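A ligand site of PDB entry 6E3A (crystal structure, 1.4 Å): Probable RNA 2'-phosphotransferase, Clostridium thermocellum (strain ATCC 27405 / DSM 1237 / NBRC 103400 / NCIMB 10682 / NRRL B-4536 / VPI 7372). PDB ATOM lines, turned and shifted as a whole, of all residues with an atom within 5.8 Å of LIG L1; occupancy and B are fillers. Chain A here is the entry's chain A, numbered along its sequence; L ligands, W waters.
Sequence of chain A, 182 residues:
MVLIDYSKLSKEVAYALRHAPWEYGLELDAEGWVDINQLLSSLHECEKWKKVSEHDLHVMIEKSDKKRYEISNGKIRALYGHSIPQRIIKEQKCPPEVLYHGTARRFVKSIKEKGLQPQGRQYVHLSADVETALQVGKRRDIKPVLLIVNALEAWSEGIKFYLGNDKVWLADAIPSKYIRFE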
ATOM      1  N   ARG A  18      13.644   3.753  -3.919  1.00  0.00           N
ATOM      2  CA  ARG A  18      12.682   3.183  -2.980  1.00  0.00           C
ATOM      3  C   ARG A  18      11.457   4.054  -2.763  1.00  0.00           C
ATOM      4  O   ARG A  18      10.374   3.541  -2.451  1.00  0.00           O
ATOM      5  CB  ARG A  18      13.313   2.986  -1.585  1.00  0.00           C
ATOM      6  CG  ARG A  18      14.461   1.956  -1.493  1.00  0.00           C
ATOM      7  CD  ARG A  18      15.000   2.036  -0.098  1.00  0.00           C
ATOM      8  NE  ARG A  18      16.060   0.985   0.080  1.00  0.00           N
ATOM      9  CZ  ARG A  18      16.869   0.952   1.140  1.00  0.00           C
ATOM     10  NH1 ARG A  18      16.754   1.826   2.146  1.00  0.00           N
ATOM     11  NH2 ARG A  18      17.784  -0.058   1.243  1.00  0.00           N
ATOM     12  N   LYS A  66      26.050  -3.416   2.844  1.00  0.00           N
ATOM     13  CA  LYS A  66      24.780  -4.082   2.622  1.00  0.00           C
ATOM     14  C   LYS A  66      24.540  -4.152   1.132  1.00  0.00           C
ATOM     15  O   LYS A  66      24.849  -3.209   0.399  1.00  0.00           O
ATOM     16  CB  LYS A  66      23.606  -3.273   3.237  1.00  0.00           C
ATOM     17  CG  LYS A  66      23.612  -3.292   4.750  1.00  0.00           C
ATOM     18  CD  LYS A  66      22.471  -2.418   5.264  1.00  0.00           C
ATOM     19  CE  LYS A  66      22.361  -2.488   6.736  1.00  0.00           C
ATOM     20  NZ  LYS A  66      21.322  -1.584   7.269  1.00  0.00           N
ATOM     21  N   ARG A  68      22.242  -3.351  -1.117  1.00  0.00           N
ATOM     22  CA  ARG A  68      20.972  -2.631  -1.269  1.00  0.00           C
ATOM     23  C   ARG A  68      20.495  -2.633  -2.702  1.00  0.00           C
ATOM     24  O   ARG A  68      19.269  -2.553  -2.961  1.00  0.00           O
ATOM     25  CB  ARG A  68      21.168  -1.169  -0.828  1.00  0.00           C
ATOM     26  CG  ARG A  68      21.433  -1.051   0.642  1.00  0.00           C
ATOM     27  CD  ARG A  68      21.509   0.423   1.062  1.00  0.00           C
ATOM     28  NE  ARG A  68      21.567   0.604   2.500  1.00  0.00           N
ATOM     29  CZ  ARG A  68      22.647   0.773   3.247  1.00  0.00           C
ATOM     30  NH1 ARG A  68      23.866   0.725   2.659  1.00  0.00           N
ATOM     31  NH2 ARG A  68      22.575   0.917   4.559  1.00  0.00           N
ATOM     32  N   TYR A  80      15.004  -3.900  -1.771  1.00  0.00           N
ATOM     33  CA  TYR A  80      14.043  -3.884  -0.672  1.00  0.00           C
ATOM     34  C   TYR A  80      13.856  -2.429  -0.285  1.00  0.00           C
ATOM     35  O   TYR A  80      14.433  -1.502  -0.870  1.00  0.00           O
ATOM     36  CB  TYR A  80      14.517  -4.766   0.484  1.00  0.00           C
ATOM     37  CG  TYR A  80      15.819  -4.303   1.119  1.00  0.00           C
ATOM     38  CD1 TYR A  80      17.059  -4.890   0.698  1.00  0.00           C
ATOM     39  CD2 TYR A  80      15.840  -3.334   2.167  1.00  0.00           C
ATOM     40  CE1 TYR A  80      18.251  -4.484   1.289  1.00  0.00           C
ATOM     41  CE2 TYR A  80      17.061  -2.921   2.741  1.00  0.00           C
ATOM     42  CZ  TYR A  80      18.260  -3.486   2.251  1.00  0.00           C
ATOM     43  OH  TYR A  80      19.419  -3.046   2.858  1.00  0.00           O
ATOM     44  N   GLY A  81      13.002  -2.228   0.698  1.00  0.00           N
ATOM     45  CA  GLY A  81      12.846  -0.909   1.287  1.00  0.00           C
ATOM     46  C   GLY A  81      11.790  -0.001   0.667  1.00  0.00           C
ATOM     47  O   GLY A  81      11.589   1.100   1.190  1.00  0.00           O
ATOM     48  N   HIS A 101      13.576  -9.999  13.919  1.00  0.00           N
ATOM     49  CA  HIS A 101      13.215  -8.628  13.585  1.00  0.00           C
ATOM     50  C   HIS A 101      13.635  -7.796  14.783  1.00  0.00           C
ATOM     51  O   HIS A 101      13.193  -8.051  15.901  1.00  0.00           O
ATOM     52  CB  HIS A 101      11.709  -8.488  13.344  1.00  0.00           C
ATOM     53  CG  HIS A 101      11.294  -7.076  13.062  1.00  0.00           C
ATOM     54  ND1 HIS A 101      11.283  -6.540  11.785  1.00  0.00           N
ATOM     55  CD2 HIS A 101      10.920  -6.079  13.894  1.00  0.00           C
ATOM     56  CE1 HIS A 101      10.884  -5.271  11.846  1.00  0.00           C
ATOM     57  NE2 HIS A 101      10.668  -4.969  13.119  1.00  0.00           N
ATOM     58  N   GLY A 102      14.532  -6.849  14.569  1.00  0.00           N
ATOM     59  CA  GLY A 102      14.945  -5.932  15.630  1.00  0.00           C
ATOM     60  C   GLY A 102      14.101  -4.644  15.580  1.00  0.00           C
ATOM     61  O   GLY A 102      13.862  -4.131  14.507  1.00  0.00           O
ATOM     62  N   THR A 103      13.686  -4.171  16.764  1.00  0.00           N
ATOM     63  CA  THR A 103      12.782  -3.017  16.812  1.00  0.00           C
ATOM     64  C   THR A 103      13.142  -2.135  17.999  1.00  0.00           C
ATOM     65  O   THR A 103      14.036  -2.460  18.792  1.00  0.00           O
ATOM     66  CB  THR A 103      11.295  -3.447  16.768  1.00  0.00           C
ATOM     67  OG1 THR A 103      10.508  -2.255  16.538  1.00  0.00           O
ATOM     68  CG2 THR A 103      10.869  -4.115  18.026  1.00  0.00           C
ATOM     69  N   ALA A 104      12.404  -1.034  18.129  1.00  0.00           N
ATOM     70  CA  ALA A 104      12.563  -0.107  19.240  1.00  0.00           C
ATOM     71  C   ALA A 104      11.633  -0.519  20.382  1.00  0.00           C
ATOM     72  O   ALA A 104      10.531  -1.027  20.135  1.00  0.00           O
ATOM     73  CB  ALA A 104      12.169   1.294  18.807  1.00  0.00           C
ATOM     74  N   PHE A 107       7.874   0.485  20.255  1.00  0.00           N
ATOM     75  CA  PHE A 107       6.928  -0.147  19.337  1.00  0.00           C
ATOM     76  C   PHE A 107       6.417  -1.505  19.820  1.00  0.00           C
ATOM     77  O   PHE A 107       5.532  -2.084  19.166  1.00  0.00           O
ATOM     78  CB  PHE A 107       7.545  -0.315  17.946  1.00  0.00           C
ATOM     79  CG  PHE A 107       7.847   0.985  17.246  1.00  0.00           C
ATOM     80  CD1 PHE A 107       7.024   2.097  17.400  1.00  0.00           C
ATOM     81  CD2 PHE A 107       8.928   1.078  16.353  1.00  0.00           C
ATOM     82  CE1 PHE A 107       7.302   3.278  16.718  1.00  0.00           C
ATOM     83  CE2 PHE A 107       9.198   2.245  15.686  1.00  0.00           C
ATOM     84  CZ  PHE A 107       8.369   3.363  15.843  1.00  0.00           C
ATOM     85  N   SER A 110       2.596  -2.188  20.590  1.00  0.00           N
ATOM     86  CA  SER A 110       1.768  -2.222  19.383  1.00  0.00           C
ATOM     87  C   SER A 110       2.051  -3.486  18.558  1.00  0.00           C
ATOM     88  O   SER A 110       1.115  -4.067  17.991  1.00  0.00           O
ATOM     89  CB  SER A 110       2.038  -0.972  18.567  1.00  0.00           C
ATOM     90  OG  SER A 110       1.236  -0.952  17.389  1.00  0.00           O
ATOM     91  N   ILE A 111       3.315  -3.921  18.461  1.00  0.00           N
ATOM     92  CA  ILE A 111       3.564  -5.157  17.727  1.00  0.00           C
ATOM     93  C   ILE A 111       2.943  -6.365  18.449  1.00  0.00           C
ATOM     94  O   ILE A 111       2.393  -7.280  17.797  1.00  0.00           O
ATOM     95  CB  ILE A 111       5.068  -5.339  17.521  1.00  0.00           C
ATOM     96  CG1 ILE A 111       5.625  -4.238  16.642  1.00  0.00           C
ATOM     97  CG2 ILE A 111       5.330  -6.678  16.815  1.00  0.00           C
ATOM     98  CD1 ILE A 111       7.198  -4.059  16.778  1.00  0.00           C
ATOM     99  N   LYS A 114      -0.859  -6.150  17.442  1.00  0.00           N
ATOM    100  CA  LYS A 114      -1.251  -6.160  16.042  1.00  0.00           C
ATOM    101  C   LYS A 114      -0.386  -7.039  15.156  1.00  0.00           C
ATOM    102  O   LYS A 114      -0.705  -7.192  13.968  1.00  0.00           O
ATOM    103  CB  LYS A 114      -1.231  -4.736  15.438  1.00  0.00           C
ATOM    104  CG  LYS A 114      -2.170  -3.815  16.174  1.00  0.00           C
ATOM    105  CD  LYS A 114      -1.969  -2.417  15.720  1.00  0.00           C
ATOM    106  CE  LYS A 114      -3.110  -1.552  16.252  1.00  0.00           C
ATOM    107  NZ  LYS A 114      -2.970  -0.122  15.823  1.00  0.00           N
ATOM    108  N   GLY A 115       0.710  -7.606  15.691  1.00  0.00           N
ATOM    109  CA  GLY A 115       1.700  -8.245  14.830  1.00  0.00           C
ATOM    110  C   GLY A 115       2.610  -7.249  14.092  1.00  0.00           C
ATOM    111  O   GLY A 115       2.448  -6.029  14.217  1.00  0.00           O
ATOM    112  N   LEU A 116       3.545  -7.765  13.324  1.00  0.00           N
ATOM    113  CA  LEU A 116       4.402  -6.904  12.517  1.00  0.00           C
ATOM    114  C   LEU A 116       3.636  -6.411  11.310  1.00  0.00           C
ATOM    115  O   LEU A 116       3.005  -7.188  10.601  1.00  0.00           O
ATOM    116  CB  LEU A 116       5.682  -7.619  12.078  1.00  0.00           C
ATOM    117  CG  LEU A 116       6.722  -7.766  13.202  1.00  0.00           C
ATOM    118  CD1 LEU A 116       7.766  -8.788  12.745  1.00  0.00           C
ATOM    119  CD2 LEU A 116       7.412  -6.431  13.522  1.00  0.00           C
ATOM    120  N   GLN A 117       3.683  -5.081  11.061  1.00  0.00           N
ATOM    121  CA  GLN A 117       2.990  -4.461   9.921  1.00  0.00           C
ATOM    122  C   GLN A 117       4.030  -3.809   9.028  1.00  0.00           C
ATOM    123  O   GLN A 117       5.103  -3.393   9.507  1.00  0.00           O
ATOM    124  CB  GLN A 117       1.963  -3.407  10.407  1.00  0.00           C
ATOM    125  CG  GLN A 117       0.795  -4.071  11.154  1.00  0.00           C
ATOM    126  CD  GLN A 117      -0.208  -4.715  10.205  1.00  0.00           C
ATOM    127  OE1 GLN A 117      -0.270  -4.389   9.022  1.00  0.00           O
ATOM    128  NE2 GLN A 117      -0.964  -5.675  10.709  1.00  0.00           N
ATOM    129  N   PRO A 118       3.743  -3.647   7.730  1.00  0.00           N
ATOM    130  CA  PRO A 118       4.713  -2.985   6.828  1.00  0.00           C
ATOM    131  C   PRO A 118       4.902  -1.525   7.133  1.00  0.00           C
ATOM    132  O   PRO A 118       5.978  -1.008   6.767  1.00  0.00           O
ATOM    133  CB  PRO A 118       4.133  -3.224   5.439  1.00  0.00           C
ATOM    134  CG  PRO A 118       3.117  -4.338   5.609  1.00  0.00           C
ATOM    135  CD  PRO A 118       2.600  -4.249   7.032  1.00  0.00           C
ATOM    136  N   GLN A 119       3.930  -0.847   7.757  1.00  0.00           N
ATOM    137  CA  GLN A 119       4.072   0.557   8.178  1.00  0.00           C
ATOM    138  C   GLN A 119       4.293   1.435   6.960  1.00  0.00           C
ATOM    139  O   GLN A 119       3.414   1.477   6.081  1.00  0.00           O
ATOM    140  CB  GLN A 119       5.140   0.677   9.291  1.00  0.00           C
ATOM    141  CG  GLN A 119       4.898  -0.194  10.546  1.00  0.00           C
ATOM    142  CD  GLN A 119       3.624   0.153  11.226  1.00  0.00           C
ATOM    143  OE1 GLN A 119       2.524  -0.152  10.734  1.00  0.00           O
ATOM    144  NE2 GLN A 119       3.712   0.817  12.381  1.00  0.00           N
ATOM    145  N   GLY A 120       5.409   2.105   6.851  1.00  0.00           N
ATOM    146  CA  GLY A 120       5.585   2.950   5.704  1.00  0.00           C
ATOM    147  C   GLY A 120       6.116   2.220   4.464  1.00  0.00           C
ATOM    148  O   GLY A 120       6.159   2.821   3.379  1.00  0.00           O
ATOM    149  N   ARG A 121       6.434   0.920   4.552  1.00  0.00           N
ATOM    150  CA  ARG A 121       6.973   0.214   3.403  1.00  0.00           C
ATOM    151  C   ARG A 121       5.910  -0.724   2.841  1.00  0.00           C
ATOM    152  O   ARG A 121       4.804  -0.872   3.391  1.00  0.00           O
ATOM    153  CB  ARG A 121       8.187  -0.571   3.833  1.00  0.00           C
ATOM    154  CG  ARG A 121       9.035   0.181   4.796  1.00  0.00           C
ATOM    155  CD  ARG A 121      10.432   0.340   4.354  1.00  0.00           C
ATOM    156  NE  ARG A 121      11.274   1.011   5.321  1.00  0.00           N
ATOM    157  CZ  ARG A 121      12.344   1.714   5.014  1.00  0.00           C
ATOM    158  NH1 ARG A 121      12.718   1.899   3.745  1.00  0.00           N
ATOM    159  NH2 ARG A 121      12.999   2.259   6.022  1.00  0.00           N
ATOM    160  N   HIS A 125      10.035  -6.161   6.871  1.00  0.00           N
ATOM    161  CA  HIS A 125      11.422  -6.586   6.627  1.00  0.00           C
ATOM    162  C   HIS A 125      11.937  -7.385   7.816  1.00  0.00           C
ATOM    163  O   HIS A 125      11.756  -6.998   8.977  1.00  0.00           O
ATOM    164  CB  HIS A 125      12.347  -5.366   6.417  1.00  0.00           C
ATOM    165  CG  HIS A 125      12.111  -4.625   5.145  1.00  0.00           C
ATOM    166  ND1 HIS A 125      10.875  -4.118   4.764  1.00  0.00           N
ATOM    167  CD2 HIS A 125      12.969  -4.311   4.130  1.00  0.00           C
ATOM    168  CE1 HIS A 125      10.980  -3.563   3.558  1.00  0.00           C
ATOM    169  NE2 HIS A 125      12.252  -3.641   3.147  1.00  0.00           N
ATOM    170  N   LEU A 126      12.604  -8.506   7.516  1.00  0.00           N
ATOM    171  CA  LEU A 126      13.111  -9.415   8.548  1.00  0.00           C
ATOM    172  C   LEU A 126      14.593  -9.710   8.284  1.00  0.00           C
ATOM    173  O   LEU A 126      15.085  -9.561   7.147  1.00  0.00           O
ATOM    174  CB  LEU A 126      12.357 -10.743   8.520  1.00  0.00           C
ATOM    175  CG  LEU A 126      10.843 -10.589   8.644  1.00  0.00           C
ATOM    176  CD1 LEU A 126      10.179 -11.953   8.378  1.00  0.00           C
ATOM    177  CD2 LEU A 126      10.485 -10.104  10.015  1.00  0.00           C
ATOM    178  N   VAL A 136      19.386  -3.487  12.872  1.00  0.00           N
ATOM    179  CA  VAL A 136      18.177  -2.816  12.384  1.00  0.00           C
ATOM    180  C   VAL A 136      17.553  -2.020  13.508  1.00  0.00           C
ATOM    181  O   VAL A 136      17.154  -0.852  13.316  1.00  0.00           O
ATOM    182  CB  VAL A 136      17.158  -3.838  11.838  1.00  0.00           C
ATOM    183  CG1 VAL A 136      15.829  -3.151  11.477  1.00  0.00           C
ATOM    184  CG2 VAL A 136      17.730  -4.572  10.598  1.00  0.00           C
ATOM    185  N   ARG A 139      18.970   1.443  14.727  1.00  0.00           N
ATOM    186  CA  ARG A 139      18.634   2.654  14.000  1.00  0.00           C
ATOM    187  C   ARG A 139      17.670   3.535  14.771  1.00  0.00           C
ATOM    188  O   ARG A 139      17.651   4.749  14.541  1.00  0.00           O
ATOM    189  CB  ARG A 139      18.059   2.299  12.621  1.00  0.00           C
ATOM    190  CG  ARG A 139      19.132   1.806  11.646  1.00  0.00           C
ATOM    191  CD  ARG A 139      18.554   0.882  10.608  1.00  0.00           C
ATOM    192  NE  ARG A 139      17.432   1.458   9.808  1.00  0.00           N
ATOM    193  CZ  ARG A 139      16.145   1.060   9.889  1.00  0.00           C
ATOM    194  NH1 ARG A 139      15.762   0.179  10.807  1.00  0.00           N
ATOM    195  NH2 ARG A 139      15.233   1.596   9.044  1.00  0.00           N
ATOM    196  N   ARG A 140      16.913   2.965  15.695  1.00  0.00           N
ATOM    197  CA  ARG A 140      15.889   3.713  16.442  1.00  0.00           C
ATOM    198  C   ARG A 140      16.048   3.639  17.946  1.00  0.00           C
ATOM    199  O   ARG A 140      15.380   4.399  18.646  1.00  0.00           O
ATOM    200  CB  ARG A 140      14.494   3.164  16.117  1.00  0.00           C
ATOM    201  CG  ARG A 140      13.958   3.590  14.740  1.00  0.00           C
ATOM    202  CD  ARG A 140      12.523   3.176  14.516  1.00  0.00           C
ATOM    203  NE  ARG A 140      12.044   3.605  13.221  1.00  0.00           N
ATOM    204  CZ  ARG A 140      12.275   2.957  12.065  1.00  0.00           C
ATOM    205  NH1 ARG A 140      12.990   1.835  12.058  1.00  0.00           N
ATOM    206  NH2 ARG A 140      11.779   3.453  10.938  1.00  0.00           N
ATOM    207  N   VAL A 168      18.098 -10.005   4.220  1.00  0.00           N
ATOM    208  CA  VAL A 168      16.868  -9.209   4.366  1.00  0.00           C
ATOM    209  C   VAL A 168      15.773 -10.019   3.710  1.00  0.00           C
ATOM    210  O   VAL A 168      15.777 -10.213   2.493  1.00  0.00           O
ATOM    211  CB  VAL A 168      16.975  -7.856   3.684  1.00  0.00           C
ATOM    212  CG1 VAL A 168      15.598  -7.121   3.849  1.00  0.00           C
ATOM    213  CG2 VAL A 168      18.023  -7.017   4.274  1.00  0.00           C
HETATM  214  C1  LIG L   1       7.894  -1.187  13.558  1.00  0.00           C
HETATM  215  C2  LIG L   1      17.053  -0.597   6.687  1.00  0.00           C
HETATM  216  C3  LIG L   1       4.225  -0.350  15.759  1.00  0.00           C
HETATM  217  C4  LIG L   1       8.954  -1.908  13.084  1.00  0.00           C
HETATM  218  C5  LIG L   1      17.077  -1.792   7.711  1.00  0.00           C
HETATM  219  C6  LIG L   1      10.021  -0.770  12.716  1.00  0.00           C
HETATM  220  C7  LIG L   1      15.944  -2.720   7.140  1.00  0.00           C
HETATM  221  C8  LIG L   1       5.540  -1.505  14.283  1.00  0.00           C
HETATM  222  C9  LIG L   1       9.195   0.257  12.222  1.00  0.00           C
HETATM  223  C10 LIG L   1      15.081  -1.902   6.450  1.00  0.00           C
HETATM  224  C11 LIG L   1       4.556  -2.417  14.017  1.00  0.00           C
HETATM  225  C12 LIG L   1       9.181   0.280  10.688  1.00  0.00           C
HETATM  226  C13 LIG L   1      13.711  -1.699   7.020  1.00  0.00           C
HETATM  227  C14 LIG L   1       3.337  -2.276  14.719  1.00  0.00           C
HETATM  228  C15 LIG L   1       6.299  -2.970  12.828  1.00  0.00           C
HETATM  229  N1  LIG L   1       3.225  -1.196  15.537  1.00  0.00           N
HETATM  230  N2  LIG L   1       5.404  -0.460  15.127  1.00  0.00           N
HETATM  231  N3  LIG L   1       2.255  -3.162  14.575  1.00  0.00           N
HETATM  232  N4  LIG L   1       5.030  -3.306  13.098  1.00  0.00           N
HETATM  233  N5  LIG L   1       6.607  -1.874  13.504  1.00  0.00           N
HETATM  234  O1  LIG L   1      12.228   1.426   8.818  1.00  0.00           O
HETATM  235  O2  LIG L   1      12.447  -3.162   9.456  1.00  0.00           O
HETATM  236  O3  LIG L   1      18.037   1.398   4.640  1.00  0.00           O
HETATM  237  O4  LIG L   1      10.069   0.695   7.866  1.00  0.00           O
HETATM  238  O5  LIG L   1       9.479  -2.768  14.108  1.00  0.00           O
HETATM  239  O6  LIG L   1      18.291  -2.318   7.834  1.00  0.00           O
HETATM  240  O7  LIG L   1      13.142  -1.063  10.731  1.00  0.00           O
HETATM  241  O8  LIG L   1      19.916   0.351   5.819  1.00  0.00           O
HETATM  242  O9  LIG L   1      11.442  -1.036   8.903  1.00  0.00           O
HETATM  243  O10 LIG L   1      10.723  -0.345  13.923  1.00  0.00           O
HETATM  244  O11 LIG L   1      16.493  -3.752   6.241  1.00  0.00           O
HETATM  245  O12 LIG L   1      19.259  -0.578   3.576  1.00  0.00           O
HETATM  246  O13 LIG L   1       7.757  -0.059  12.573  1.00  0.00           O
HETATM  247  O14 LIG L   1      15.795  -0.455   6.357  1.00  0.00           O
HETATM  248  O15 LIG L   1      17.782  -0.954   5.496  1.00  0.00           O
HETATM  249  O16 LIG L   1      10.440   0.862  10.340  1.00  0.00           O
HETATM  250  O17 LIG L   1      13.895  -1.265   8.366  1.00  0.00           O
HETATM  251  P1  LIG L   1      11.060   0.536   8.914  1.00  0.00           P
HETATM  252  P2  LIG L   1      12.763  -1.717   9.457  1.00  0.00           P
HETATM  253  P3  LIG L   1      18.816   0.100   4.861  1.00  0.00           P
HETATM  254  N1  LG2 L   2      24.561   4.357   5.141  1.00  0.00           N
HETATM  255  C1  LG2 L   2      23.436   4.618   5.874  1.00  0.00           C
HETATM  256  N2  LG2 L   2      22.196   4.608   5.278  1.00  0.00           N
HETATM  257  C2  LG2 L   2      22.075   4.347   3.943  1.00  0.00           C
HETATM  258  C3  LG2 L   2      23.199   4.076   3.228  1.00  0.00           C
HETATM  259  C4  LG2 L   2      24.453   4.090   3.849  1.00  0.00           C
HETATM  260  N3  LG2 L   2      25.734   3.834   3.271  1.00  0.00           N
HETATM  261  N4  LG2 L   2      22.839   3.845   1.965  1.00  0.00           N
HETATM  262  C5  LG2 L   2      21.514   3.940   1.878  1.00  0.00           C
HETATM  263  N5  LG2 L   2      21.034   4.228   3.077  1.00  0.00           N
HETATM  264  C6  LG2 L   2      19.630   4.422   3.339  1.00  0.00           C
HETATM  265  C7  LG2 L   2      19.256   4.694   4.568  1.00  0.00           C
HETATM  266  O1  LG2 L   2      19.036   3.540   5.345  1.00  0.00           O
HETATM  267  C8  LG2 L   2      17.892   5.392   4.301  1.00  0.00           C
HETATM  268  O2  LG2 L   2      17.006   4.450   3.924  1.00  0.00           O
HETATM  269  P1  LG2 L   2      15.363   4.675   4.067  1.00  0.00           P
HETATM  270  O3  LG2 L   2      15.080   6.154   3.824  1.00  0.00           O
HETATM  271  O4  LG2 L   2      14.714   3.739   3.031  1.00  0.00           O
HETATM  272  O5  LG2 L   2      14.983   4.331   5.479  1.00  0.00           O
HETATM  273  C9  LG2 L   2      18.224   6.327   3.094  1.00  0.00           C
HETATM  274  O6  LG2 L   2      19.368   5.871   2.633  1.00  0.00           O
HETATM  275  C10 LG2 L   2      18.468   7.762   3.534  1.00  0.00           C
HETATM  276  O7  LG2 L   2      19.091   7.726   4.786  1.00  0.00           O
HETATM  277  P2  LG2 L   2      19.239   9.147   5.596  1.00  0.00           P
HETATM  278  O8  LG2 L   2      20.233   8.945   6.713  1.00  0.00           O
HETATM  279  O9  LG2 L   2      17.914   9.557   6.160  1.00  0.00           O
HETATM  280  O10 LG2 L   2      19.794  10.209   4.451  1.00  0.00           O
HETATM  281  P3  LG2 L   2      19.965  11.894   4.611  1.00  0.00           P
HETATM  282  O11 LG2 L   2      19.273  12.371   5.874  1.00  0.00           O
HETATM  283  O12 LG2 L   2      21.439  12.254   4.687  1.00  0.00           O
HETATM  284  O13 LG2 L   2      19.308  12.591   3.253  1.00  0.00           O
HETATM  285  C11 LG2 L   2      18.397  12.245   1.058  1.00  0.00           C
HETATM  286  C12 LG2 L   2      19.621  12.073   1.954  1.00  0.00           C
HETATM  287  C13 LG2 L   2      18.720  11.937  -0.360  1.00  0.00           C
HETATM  288  C14 LG2 L   2      17.342  11.270   1.508  1.00  0.00           C
HETATM  289  C15 LG2 L   2      17.892  13.707   1.178  1.00  0.00           C
HETATM  290  O14 LG2 L   2      18.910  14.566   0.835  1.00  0.00           O
HETATM  291  C16 LG2 L   2      16.639  13.960   0.266  1.00  0.00           C
HETATM  292  O15 LG2 L   2      15.537  13.576   0.608  1.00  0.00           O
HETATM  293  N6  LG2 L   2      16.801  14.706  -1.044  1.00  0.00           N
HETATM  294  C17 LG2 L   2      15.598  14.962  -1.953  1.00  0.00           C
HETATM  295  C18 LG2 L   2      16.070  15.310  -3.370  1.00  0.00           C
HETATM  296  C19 LG2 L   2      17.379  16.109  -3.260  1.00  0.00           C
HETATM  297  O16 LG2 L   2      17.394  17.164  -2.695  1.00  0.00           O
HETATM  298  N7  LG2 L   2      18.568  15.586  -3.830  1.00  0.00           N
HETATM  299  C20 LG2 L   2      19.836  16.306  -3.761  1.00  0.00           C
HETATM  300  C21 LG2 L   2      19.745  17.567  -4.654  1.00  0.00           C
HETATM  301  S1  LG2 L   2      21.395  18.365  -4.530  1.00  0.00           S
HETATM  302  O   HOH W   1       7.937   2.496   8.108  1.00  0.00           O
HETATM  303  O   HOH W   2      20.467  -2.040   9.804  1.00  0.00           O
HETATM  304  O   HOH W   3      15.618  -6.030   7.388  1.00  0.00           O
HETATM  305  O   HOH W   4      13.049  -1.756  13.370  1.00  0.00           O
HETATM  306  O   HOH W   5       7.676  -4.287  10.344  1.00  0.00           O
HETATM  307  O   HOH W   6      13.914  -5.465   9.616  1.00  0.00           O
HETATM  308  O   HOH W   7      19.161  -3.857   5.598  1.00  0.00           O
HETATM  309  O   HOH W   8      20.057   2.101   7.645  1.00  0.00           O
HETATM  310  O   HOH W   9       9.868  -3.819   8.545  1.00  0.00           O
HETATM  311  O   HOH W  10       8.570  -1.677   7.314  1.00  0.00           O
HETATM  312  O   HOH W  11       6.188   2.159  13.240  1.00  0.00           O
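Water W8 lies within hydrogen-bond range of O8 of LIG L1 (2.5 Å), O1 of LG2 L2 (2.9 Å) and NE of Arg 139 (3.5 Å). Water W6 lies within hydrogen-bond range of the backbone carbonyl oxygen of His 125 and an oxygen (O2) of LIG L1. Water W7 lies within hydrogen-bond range of an oxygen (O11) of LIG L1 (2.7 Å) and the side-chain hydroxyl (OH) of Tyr 80 (2.9 Å). Water W11 bridges an oxygen (O13) of LIG L1 and the side-chain amide nitrogen of Gln 119. Water W9 lies within hydrogen-bond range of an oxygen (O2) of LIG L1 (2.8 Å) and the backbone NH of His 125 (2.9 Å). Water W2 bridges NZ of Lys 66 (2.7 Å) and O6 of LIG L1 (2.9 Å).
The side-chain hydroxyl (OH) of Tyr 80 lies within hydrogen-bond range of an oxygen (O12) of LIG L1. OG1 of Thr 103 sits at hydrogen-bond distance from O5 of LIG L1 (2.7 Å). A ring nitrogen (NE2) of His 101 is in hydrogen-bond range of an oxygen (O5) of LIG L1. N1 of LIG L1 sits at hydrogen-bond distance from OG of Ser 110, at 2.7 Å. The side-chain amino group (NZ) of Lys 66 lies within salt-bridge range of an oxygen (O8) of LIG L1. NE of Arg 68 is in salt-bridge range of O12 of LIG L1. NH2 of Arg 18 is in salt-bridge range of O12 of LIG L1, 2.8 Å away. NE of Arg 121 lies within salt-bridge range of O4 of LIG L1 (2.8 Å). A nitrogen (N3) of LIG L1 sits at hydrogen-bond distance from the backbone carbonyl oxygen of Gly 115. O7 of LIG L1 lies within salt-bridge range of NH1 of Arg 139, at 2.9 Å. The guanidinium group of Arg 140 lies within salt-bridge range of an oxygen (O1) of LIG L1, at 3.0 Å. The backbone NH (N) of Gln 117 is in hydrogen-bond range of a nitrogen (N4) of LIG L1 (3.0 Å). NE2 of Gln 119 is in hydrogen-bond range of N2 of LIG L1, at 3.5 Å. NH1 of Arg 68 sits close to N4 of LG2 L2 (3.4 Å). NH1 of Arg 18 is in salt-bridge range of O4 of LG2 L2. The guanidinium group (NH1) of Arg 121 lies within salt-bridge range of an oxygen (O4) of LG2 L2 (2.8 Å).
An oxygen (O3) of LIG L1 is in hydrogen-bond range of an oxygen (O1) of LG2 L2, 2.5 Å away.
O of Tyr 80 sits at hydrogen-bond distance from NE of Arg 18. ND1 of His 101 sits at hydrogen-bond distance from O of His 125 (2.9 Å). The guanidinium group (NH1) of Arg 121 lies within hydrogen-bond range of the backbone carbonyl oxygen (O) of Gly 81. The guanidinium group (NH1) of Arg 139 is in hydrogen-bond range of the backbone carbonyl oxygen (O) of Val 136 (3.0 Å). A ring nitrogen (NE2) of His 125 is in hydrogen-bond range of the backbone NH (N) of Gly 81, at 2.9 Å.
Merely in contact with LIG L1: Phe 107 (3.3 Å), Ile 111 (3.4 Å), Val 136 (3.5 Å), Leu 116 (3.7 Å), His 125 (3.8 Å) and Lys 114 (3.9 Å). Hydrophobic or aromatic side chains that line LIG L1: Tyr 80, His 101, Phe 107, Ile 111, Leu 116, His 125 and Val 136. 19 residues have an atom within 4 Å of LIG L1: Arg 18, Lys 66, Arg 68, Tyr 80, His 101, Thr 103, Phe 107, Ser 110, Ile 111, Lys 114, Gly 115, Leu 116, Gln 117, Gln 119, Arg 121, His 125, Val 136, Arg 139 and Arg 140. The nearest printed residue that does not touch LIG L1 is Val 168 (4.1 Å).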
